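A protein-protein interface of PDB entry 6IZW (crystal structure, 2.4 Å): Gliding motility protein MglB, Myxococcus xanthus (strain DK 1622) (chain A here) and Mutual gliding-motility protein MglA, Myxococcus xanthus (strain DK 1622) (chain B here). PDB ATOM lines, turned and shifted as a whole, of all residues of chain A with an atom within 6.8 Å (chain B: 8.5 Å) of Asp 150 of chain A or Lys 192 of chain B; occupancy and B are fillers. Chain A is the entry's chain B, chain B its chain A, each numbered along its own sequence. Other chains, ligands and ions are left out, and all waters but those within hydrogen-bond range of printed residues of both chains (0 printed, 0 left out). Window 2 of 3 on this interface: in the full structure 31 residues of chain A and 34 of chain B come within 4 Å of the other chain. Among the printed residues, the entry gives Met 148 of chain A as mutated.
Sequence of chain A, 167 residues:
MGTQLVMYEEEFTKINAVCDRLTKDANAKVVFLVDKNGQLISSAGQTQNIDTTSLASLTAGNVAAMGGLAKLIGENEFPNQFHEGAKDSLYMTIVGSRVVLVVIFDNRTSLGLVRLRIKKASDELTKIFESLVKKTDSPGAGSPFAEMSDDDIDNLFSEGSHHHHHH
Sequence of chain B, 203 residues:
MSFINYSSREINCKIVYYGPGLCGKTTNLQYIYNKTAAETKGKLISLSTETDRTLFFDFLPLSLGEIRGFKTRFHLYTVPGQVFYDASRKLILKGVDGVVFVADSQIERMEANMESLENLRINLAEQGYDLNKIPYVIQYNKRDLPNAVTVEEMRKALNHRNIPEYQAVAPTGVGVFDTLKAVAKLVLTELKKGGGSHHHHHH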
ATOM      1  N   PHE A 145     -18.753  35.321   9.482  1.00  0.00           N
ATOM      2  CA  PHE A 145     -19.236  34.241  10.321  1.00  0.00           C
ATOM      3  C   PHE A 145     -20.597  33.700   9.902  1.00  0.00           C
ATOM      4  O   PHE A 145     -20.938  32.569  10.270  1.00  0.00           O
ATOM      5  CB  PHE A 145     -19.277  34.721  11.773  1.00  0.00           C
ATOM      6  CG  PHE A 145     -17.950  35.215  12.268  1.00  0.00           C
ATOM      7  CD1 PHE A 145     -16.897  34.324  12.475  1.00  0.00           C
ATOM      8  CD2 PHE A 145     -17.741  36.569  12.522  1.00  0.00           C
ATOM      9  CE1 PHE A 145     -15.650  34.773  12.936  1.00  0.00           C
ATOM     10  CE2 PHE A 145     -16.502  37.024  12.988  1.00  0.00           C
ATOM     11  CZ  PHE A 145     -15.455  36.119  13.194  1.00  0.00           C
ATOM     12  N   ALA A 146     -21.360  34.459   9.120  1.00  0.00           N
ATOM     13  CA  ALA A 146     -22.702  34.026   8.746  1.00  0.00           C
ATOM     14  C   ALA A 146     -22.664  32.766   7.883  1.00  0.00           C
ATOM     15  O   ALA A 146     -23.431  31.822   8.114  1.00  0.00           O
ATOM     16  CB  ALA A 146     -23.424  35.157   8.020  1.00  0.00           C
ATOM     17  N   GLU A 147     -21.789  32.734   6.879  1.00  0.00           N
ATOM     18  CA  GLU A 147     -21.664  31.568   6.012  1.00  0.00           C
ATOM     19  C   GLU A 147     -20.585  30.605   6.490  1.00  0.00           C
ATOM     20  O   GLU A 147     -20.203  29.695   5.750  1.00  0.00           O
ATOM     21  CB  GLU A 147     -21.388  32.001   4.566  1.00  0.00           C
ATOM     22  N   MET A 148     -20.091  30.784   7.702  1.00  0.00           N
ATOM     23  CA  MET A 148     -19.047  29.915   8.212  1.00  0.00           C
ATOM     24  C   MET A 148     -19.615  28.620   8.786  1.00  0.00           C
ATOM     25  O   MET A 148     -20.726  28.596   9.314  1.00  0.00           O
ATOM     26  CB  MET A 148     -18.247  30.629   9.283  1.00  0.00           C
ATOM     27  CG  MET A 148     -17.065  29.835   9.751  1.00  0.00           C
ATOM     28  SD  MET A 148     -16.023  30.841  11.029  1.00  0.00           S
ATOM     29  CE  MET A 148     -15.657  32.417   9.899  1.00  0.00           C
ATOM     30  N   SER A 149     -18.851  27.537   8.679  1.00  0.00           N
ATOM     31  CA  SER A 149     -19.240  26.269   9.267  1.00  0.00           C
ATOM     32  C   SER A 149     -18.052  25.718  10.031  1.00  0.00           C
ATOM     33  O   SER A 149     -16.936  26.226   9.927  1.00  0.00           O
ATOM     34  CB  SER A 149     -19.739  25.287   8.198  1.00  0.00           C
ATOM     35  OG  SER A 149     -18.742  25.055   7.216  1.00  0.00           O
ATOM     36  N   ASP A 150     -18.300  24.685  10.832  1.00  0.00           N
ATOM     37  CA  ASP A 150     -17.247  24.211  11.720  1.00  0.00           C
ATOM     38  C   ASP A 150     -16.095  23.546  10.981  1.00  0.00           C
ATOM     39  O   ASP A 150     -15.024  23.386  11.569  1.00  0.00           O
ATOM     40  CB  ASP A 150     -17.819  23.259  12.764  1.00  0.00           C
ATOM     41  CG  ASP A 150     -18.551  23.997  13.847  1.00  0.00           C
ATOM     42  OD1 ASP A 150     -19.754  24.273  13.659  1.00  0.00           O
ATOM     43  OD2 ASP A 150     -17.911  24.346  14.867  1.00  0.00           O
ATOM     44  N   ASP A 151     -16.272  23.157   9.715  1.00  0.00           N
ATOM     45  CA  ASP A 151     -15.126  22.666   8.959  1.00  0.00           C
ATOM     46  C   ASP A 151     -14.140  23.795   8.671  1.00  0.00           C
ATOM     47  O   ASP A 151     -12.926  23.583   8.704  1.00  0.00           O
ATOM     48  CB  ASP A 151     -15.579  21.980   7.669  1.00  0.00           C
ATOM     49  CG  ASP A 151     -16.566  22.812   6.879  1.00  0.00           C
ATOM     50  OD1 ASP A 151     -17.672  23.060   7.407  1.00  0.00           O
ATOM     51  OD2 ASP A 151     -16.241  23.233   5.737  1.00  0.00           O
ATOM     52  N   ASP A 152     -14.643  25.014   8.446  1.00  0.00           N
ATOM     53  CA  ASP A 152     -13.761  26.173   8.271  1.00  0.00           C
ATOM     54  C   ASP A 152     -12.849  26.362   9.479  1.00  0.00           C
ATOM     55  O   ASP A 152     -11.672  26.706   9.336  1.00  0.00           O
ATOM     56  CB  ASP A 152     -14.601  27.434   8.028  1.00  0.00           C
ATOM     57  CG  ASP A 152     -15.213  27.470   6.623  1.00  0.00           C
ATOM     58  OD1 ASP A 152     -14.473  27.199   5.643  1.00  0.00           O
ATOM     59  OD2 ASP A 152     -16.430  27.764   6.493  1.00  0.00           O
ATOM     60  N   ILE A 153     -13.386  26.136  10.674  1.00  0.00           N
ATOM     61  CA  ILE A 153     -12.620  26.250  11.902  1.00  0.00           C
ATOM     62  C   ILE A 153     -11.677  25.061  12.055  1.00  0.00           C
ATOM     63  O   ILE A 153     -10.458  25.233  12.187  1.00  0.00           O
ATOM     64  CB  ILE A 153     -13.581  26.370  13.100  1.00  0.00           C
ATOM     65  CG1 ILE A 153     -14.241  27.758  13.133  1.00  0.00           C
ATOM     66  CG2 ILE A 153     -12.879  26.010  14.411  1.00  0.00           C
ATOM     67  CD1 ILE A 153     -15.403  27.824  14.104  1.00  0.00           C
ATOM     68  N   ASP A 154     -12.231  23.831  12.036  1.00  0.00           N
ATOM     69  CA  ASP A 154     -11.425  22.622  12.254  1.00  0.00           C
ATOM     70  C   ASP A 154     -10.277  22.491  11.246  1.00  0.00           C
ATOM     71  O   ASP A 154      -9.217  21.963  11.585  1.00  0.00           O
ATOM     72  CB  ASP A 154     -12.309  21.367  12.194  1.00  0.00           C
ATOM     73  CG  ASP A 154     -13.253  21.248  13.380  1.00  0.00           C
ATOM     74  OD1 ASP A 154     -13.156  22.059  14.332  1.00  0.00           O
ATOM     75  OD2 ASP A 154     -14.119  20.341  13.353  1.00  0.00           O
ATOM     76  N   ASN A 155     -10.465  22.960  10.015  1.00  0.00           N
ATOM     77  CA  ASN A 155      -9.441  22.923   8.973  1.00  0.00           C
ATOM     78  C   ASN A 155      -8.435  24.066   9.068  1.00  0.00           C
ATOM     79  O   ASN A 155      -7.808  24.399   8.050  1.00  0.00           O
ATOM     80  CB  ASN A 155     -10.082  22.983   7.582  1.00  0.00           C
ATOM     81  CG  ASN A 155     -10.849  21.723   7.219  1.00  0.00           C
ATOM     82  OD1 ASN A 155     -10.713  20.672   7.870  1.00  0.00           O
ATOM     83  ND2 ASN A 155     -11.665  21.827   6.157  1.00  0.00           N
ATOM     84  N   ILE B   4     -12.102  42.766  14.412  1.00  0.00           N
ATOM     85  CA  ILE B   4     -12.137  42.387  12.999  1.00  0.00           C
ATOM     86  C   ILE B   4     -11.945  43.628  12.135  1.00  0.00           C
ATOM     87  O   ILE B   4     -12.731  44.581  12.202  1.00  0.00           O
ATOM     88  CB  ILE B   4     -13.431  41.648  12.630  1.00  0.00           C
ATOM     89  CG1 ILE B   4     -13.652  40.474  13.586  1.00  0.00           C
ATOM     90  CG2 ILE B   4     -13.355  41.133  11.201  1.00  0.00           C
ATOM     91  CD1 ILE B   4     -15.088  40.135  13.786  1.00  0.00           C
ATOM     92  N   ILE B  67      -9.720  31.934   7.244  1.00  0.00           N
ATOM     93  CA  ILE B  67     -11.072  31.422   7.340  1.00  0.00           C
ATOM     94  C   ILE B  67     -11.941  32.339   6.505  1.00  0.00           C
ATOM     95  O   ILE B  67     -12.093  33.523   6.842  1.00  0.00           O
ATOM     96  CB  ILE B  67     -11.599  31.367   8.785  1.00  0.00           C
ATOM     97  CG1 ILE B  67     -10.699  30.528   9.680  1.00  0.00           C
ATOM     98  CG2 ILE B  67     -12.945  30.698   8.795  1.00  0.00           C
ATOM     99  CD1 ILE B  67     -11.450  29.882  10.862  1.00  0.00           C
ATOM    100  N   LYS B 185      -9.809  27.288  18.689  1.00  0.00           N
ATOM    101  CA  LYS B 185     -11.062  26.930  18.034  1.00  0.00           C
ATOM    102  C   LYS B 185     -12.268  27.297  18.901  1.00  0.00           C
ATOM    103  O   LYS B 185     -13.307  27.702  18.371  1.00  0.00           O
ATOM    104  CB  LYS B 185     -11.074  25.452  17.653  1.00  0.00           C
ATOM    105  CG  LYS B 185      -9.884  25.057  16.796  1.00  0.00           C
ATOM    106  CD  LYS B 185     -10.038  23.703  16.147  1.00  0.00           C
ATOM    107  CE  LYS B 185     -11.007  22.792  16.873  1.00  0.00           C
ATOM    108  NZ  LYS B 185     -10.915  21.386  16.325  1.00  0.00           N
ATOM    109  N   LEU B 186     -12.149  27.205  20.234  1.00  0.00           N
ATOM    110  CA  LEU B 186     -13.234  27.687  21.084  1.00  0.00           C
ATOM    111  C   LEU B 186     -13.454  29.180  20.888  1.00  0.00           C
ATOM    112  O   LEU B 186     -14.599  29.635  20.851  1.00  0.00           O
ATOM    113  CB  LEU B 186     -12.965  27.374  22.553  1.00  0.00           C
ATOM    114  CG  LEU B 186     -13.037  25.906  22.968  1.00  0.00           C
ATOM    115  CD1 LEU B 186     -12.525  25.743  24.391  1.00  0.00           C
ATOM    116  CD2 LEU B 186     -14.439  25.376  22.879  1.00  0.00           C
ATOM    117  N   VAL B 187     -12.378  29.957  20.720  1.00  0.00           N
ATOM    118  CA  VAL B 187     -12.543  31.394  20.489  1.00  0.00           C
ATOM    119  C   VAL B 187     -13.252  31.632  19.163  1.00  0.00           C
ATOM    120  O   VAL B 187     -14.213  32.400  19.085  1.00  0.00           O
ATOM    121  CB  VAL B 187     -11.181  32.119  20.542  1.00  0.00           C
ATOM    122  CG1 VAL B 187     -11.250  33.453  19.844  1.00  0.00           C
ATOM    123  CG2 VAL B 187     -10.739  32.343  21.981  1.00  0.00           C
ATOM    124  N   LEU B 188     -12.791  30.959  18.100  1.00  0.00           N
ATOM    125  CA  LEU B 188     -13.400  31.126  16.788  1.00  0.00           C
ATOM    126  C   LEU B 188     -14.831  30.608  16.768  1.00  0.00           C
ATOM    127  O   LEU B 188     -15.668  31.137  16.038  1.00  0.00           O
ATOM    128  CB  LEU B 188     -12.562  30.421  15.722  1.00  0.00           C
ATOM    129  CG  LEU B 188     -11.222  31.078  15.429  1.00  0.00           C
ATOM    130  CD1 LEU B 188     -10.537  30.285  14.359  1.00  0.00           C
ATOM    131  CD2 LEU B 188     -11.323  32.569  15.049  1.00  0.00           C
ATOM    132  N   THR B 189     -15.137  29.592  17.571  1.00  0.00           N
ATOM    133  CA  THR B 189     -16.511  29.108  17.630  1.00  0.00           C
ATOM    134  C   THR B 189     -17.413  30.132  18.306  1.00  0.00           C
ATOM    135  O   THR B 189     -18.573  30.308  17.914  1.00  0.00           O
ATOM    136  CB  THR B 189     -16.563  27.779  18.374  1.00  0.00           C
ATOM    137  OG1 THR B 189     -15.804  26.807  17.650  1.00  0.00           O
ATOM    138  CG2 THR B 189     -18.007  27.305  18.540  1.00  0.00           C
ATOM    139  N   GLU B 190     -16.872  30.835  19.304  1.00  0.00           N
ATOM    140  CA  GLU B 190     -17.609  31.882  19.997  1.00  0.00           C
ATOM    141  C   GLU B 190     -17.947  33.028  19.058  1.00  0.00           C
ATOM    142  O   GLU B 190     -19.069  33.527  19.056  1.00  0.00           O
ATOM    143  CB  GLU B 190     -16.780  32.381  21.192  1.00  0.00           C
ATOM    144  CG  GLU B 190     -17.488  33.359  22.120  1.00  0.00           C
ATOM    145  CD  GLU B 190     -18.626  32.690  22.872  1.00  0.00           C
ATOM    146  OE1 GLU B 190     -18.583  31.442  23.010  1.00  0.00           O
ATOM    147  OE2 GLU B 190     -19.564  33.403  23.312  1.00  0.00           O
ATOM    148  N   LEU B 191     -16.983  33.477  18.261  1.00  0.00           N
ATOM    149  CA  LEU B 191     -17.286  34.537  17.305  1.00  0.00           C
ATOM    150  C   LEU B 191     -18.376  34.106  16.324  1.00  0.00           C
ATOM    151  O   LEU B 191     -19.299  34.874  16.038  1.00  0.00           O
ATOM    152  CB  LEU B 191     -16.022  34.955  16.559  1.00  0.00           C
ATOM    153  CG  LEU B 191     -14.881  35.415  17.468  1.00  0.00           C
ATOM    154  CD1 LEU B 191     -13.611  35.691  16.659  1.00  0.00           C
ATOM    155  CD2 LEU B 191     -15.311  36.644  18.248  1.00  0.00           C
ATOM    156  N   LYS B 192     -18.293  32.869  15.823  1.00  0.00           N
ATOM    157  CA  LYS B 192     -19.285  32.335  14.884  1.00  0.00           C
ATOM    158  C   LYS B 192     -20.717  32.538  15.367  1.00  0.00           C
ATOM    159  O   LYS B 192     -21.612  32.794  14.558  1.00  0.00           O
ATOM    160  CB  LYS B 192     -19.001  30.841  14.645  1.00  0.00           C
ATOM    161  CG  LYS B 192     -20.006  30.073  13.799  1.00  0.00           C
ATOM    162  CD  LYS B 192     -19.503  28.631  13.622  1.00  0.00           C
ATOM    163  CE  LYS B 192     -20.626  27.651  13.388  1.00  0.00           C
ATOM    164  NZ  LYS B 192     -21.013  27.688  11.954  1.00  0.00           N
ATOM    165  N   LYS B 193     -20.943  32.455  16.673  1.00  0.00           N
ATOM    166  CA  LYS B 193     -22.256  32.674  17.288  1.00  0.00           C
ATOM    167  C   LYS B 193     -22.703  34.142  17.244  1.00  0.00           C
ATOM    168  O   LYS B 193     -22.026  35.037  17.776  1.00  0.00           O
ATOM    169  CB  LYS B 193     -22.237  32.174  18.746  1.00  0.00           C
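Of the 11 printed residues of chain B, 7 touch a printed residue of chain A.
Printed residues of chain B that touch a printed residue of chain A: Ile 4, Ile 67, Lys 185, Leu 188, Thr 189, Leu 191 and Lys 192.
Hydrophobic or aromatic side chains of chain B that line the printed part of chain A: Ile 4, Ile 67 and Leu 191.
Printed residues of chain A that touch a printed residue of chain B: Phe 145, Met 148, Ser 149, Asp 150, Asp 152, Ile 153 and Asp 154.
Among the printed residues, Asp or Glu carboxylates within 4 Å of a Lys or Arg side-chain nitrogen of the other chain: Asp 154 of chain A with Lys 185 of chain B.
The side-chain amino group (NZ) of Lys 192 of chain B is in hydrogen-bond range of the backbone carbonyl oxygen (O) of Met 148 of chain A, at 2.8 Å.
The side-chain carboxylate (OD1) of Asp 154 of chain A lies within salt-bridge range of the side-chain amino group (NZ) of Lys 185 of chain B.
The side-chain carboxylate of Asp 152 of chain A is in hydrogen-bond range of the backbone NH of Ser 149 of chain A, at 3.3 Å.
The side-chain hydroxyl of Ser 149 of chain A lies close to the side-chain carboxylate of Asp 151 of chain A.
The backbone carbonyl oxygen (O) of Lys 185 of chain B sits at hydrogen-bond distance from the side-chain hydroxyl (OG1) of Thr 189 of chain B (2.7 Å).
Among the printed residues, pairs that only touch across the chains: Met 148 of chain A with Ile 67 of chain B (3.4 Å), Asp 150 of chain A with Lys 192 of chain B (3.5 Å), Phe 145 of chain A with Ile 4 of chain B (3.5 Å), Ser 149 of chain A with Lys 192 of chain B (3.5 Å), Asp 152 of chain A with Ile 67 of chain B (3.5 Å), Phe 145 of chain A with Leu 191 of chain B (3.6 Å), Ile 153 of chain A with Thr 189 of chain B (3.7 Å), Ile 153 of chain A with Lys 185 of chain B (3.8 Å), Ile 153 of chain A with Leu 188 of chain B (3.8 Å), Phe 145 of chain A with Lys 192 of chain B (3.9 Å) and Ile 153 of chain A with Ile 67 of chain B (3.95 Å).
Of the printed residues of chain B, Ser 149 of chain A touches Lys 192.
Of chain B, only Lys 192 (3.5 Å) comes within 4 Å of Asp 150 of chain A.
Printed residues of chain B within 4 Å of Ile 153 of chain A: Ile 67, Lys 185, Leu 188 and Thr 189.
Of the printed residues of chain A, Ile 4 of chain B touches Phe 145 (3.5 Å).
Of the printed residues of chain A, Lys 185 of chain B touches Ile 153 and Asp 154.
Of the printed residues of chain A, Leu 188 of chain B touches Ile 153 (3.8 Å).
Of chain A, only Phe 145, Met 148, Ser 149 and Asp 150 come within 4 Å of Lys 192 of chain B.
The nearest residue of chain A that does not touch Lys 192 of chain B is Ile 153 of chain A (4.2 Å).
The nearest printed residue of chain B that does not touch Ile 153 of chain A is Lys 192 of chain B (4.2 Å).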
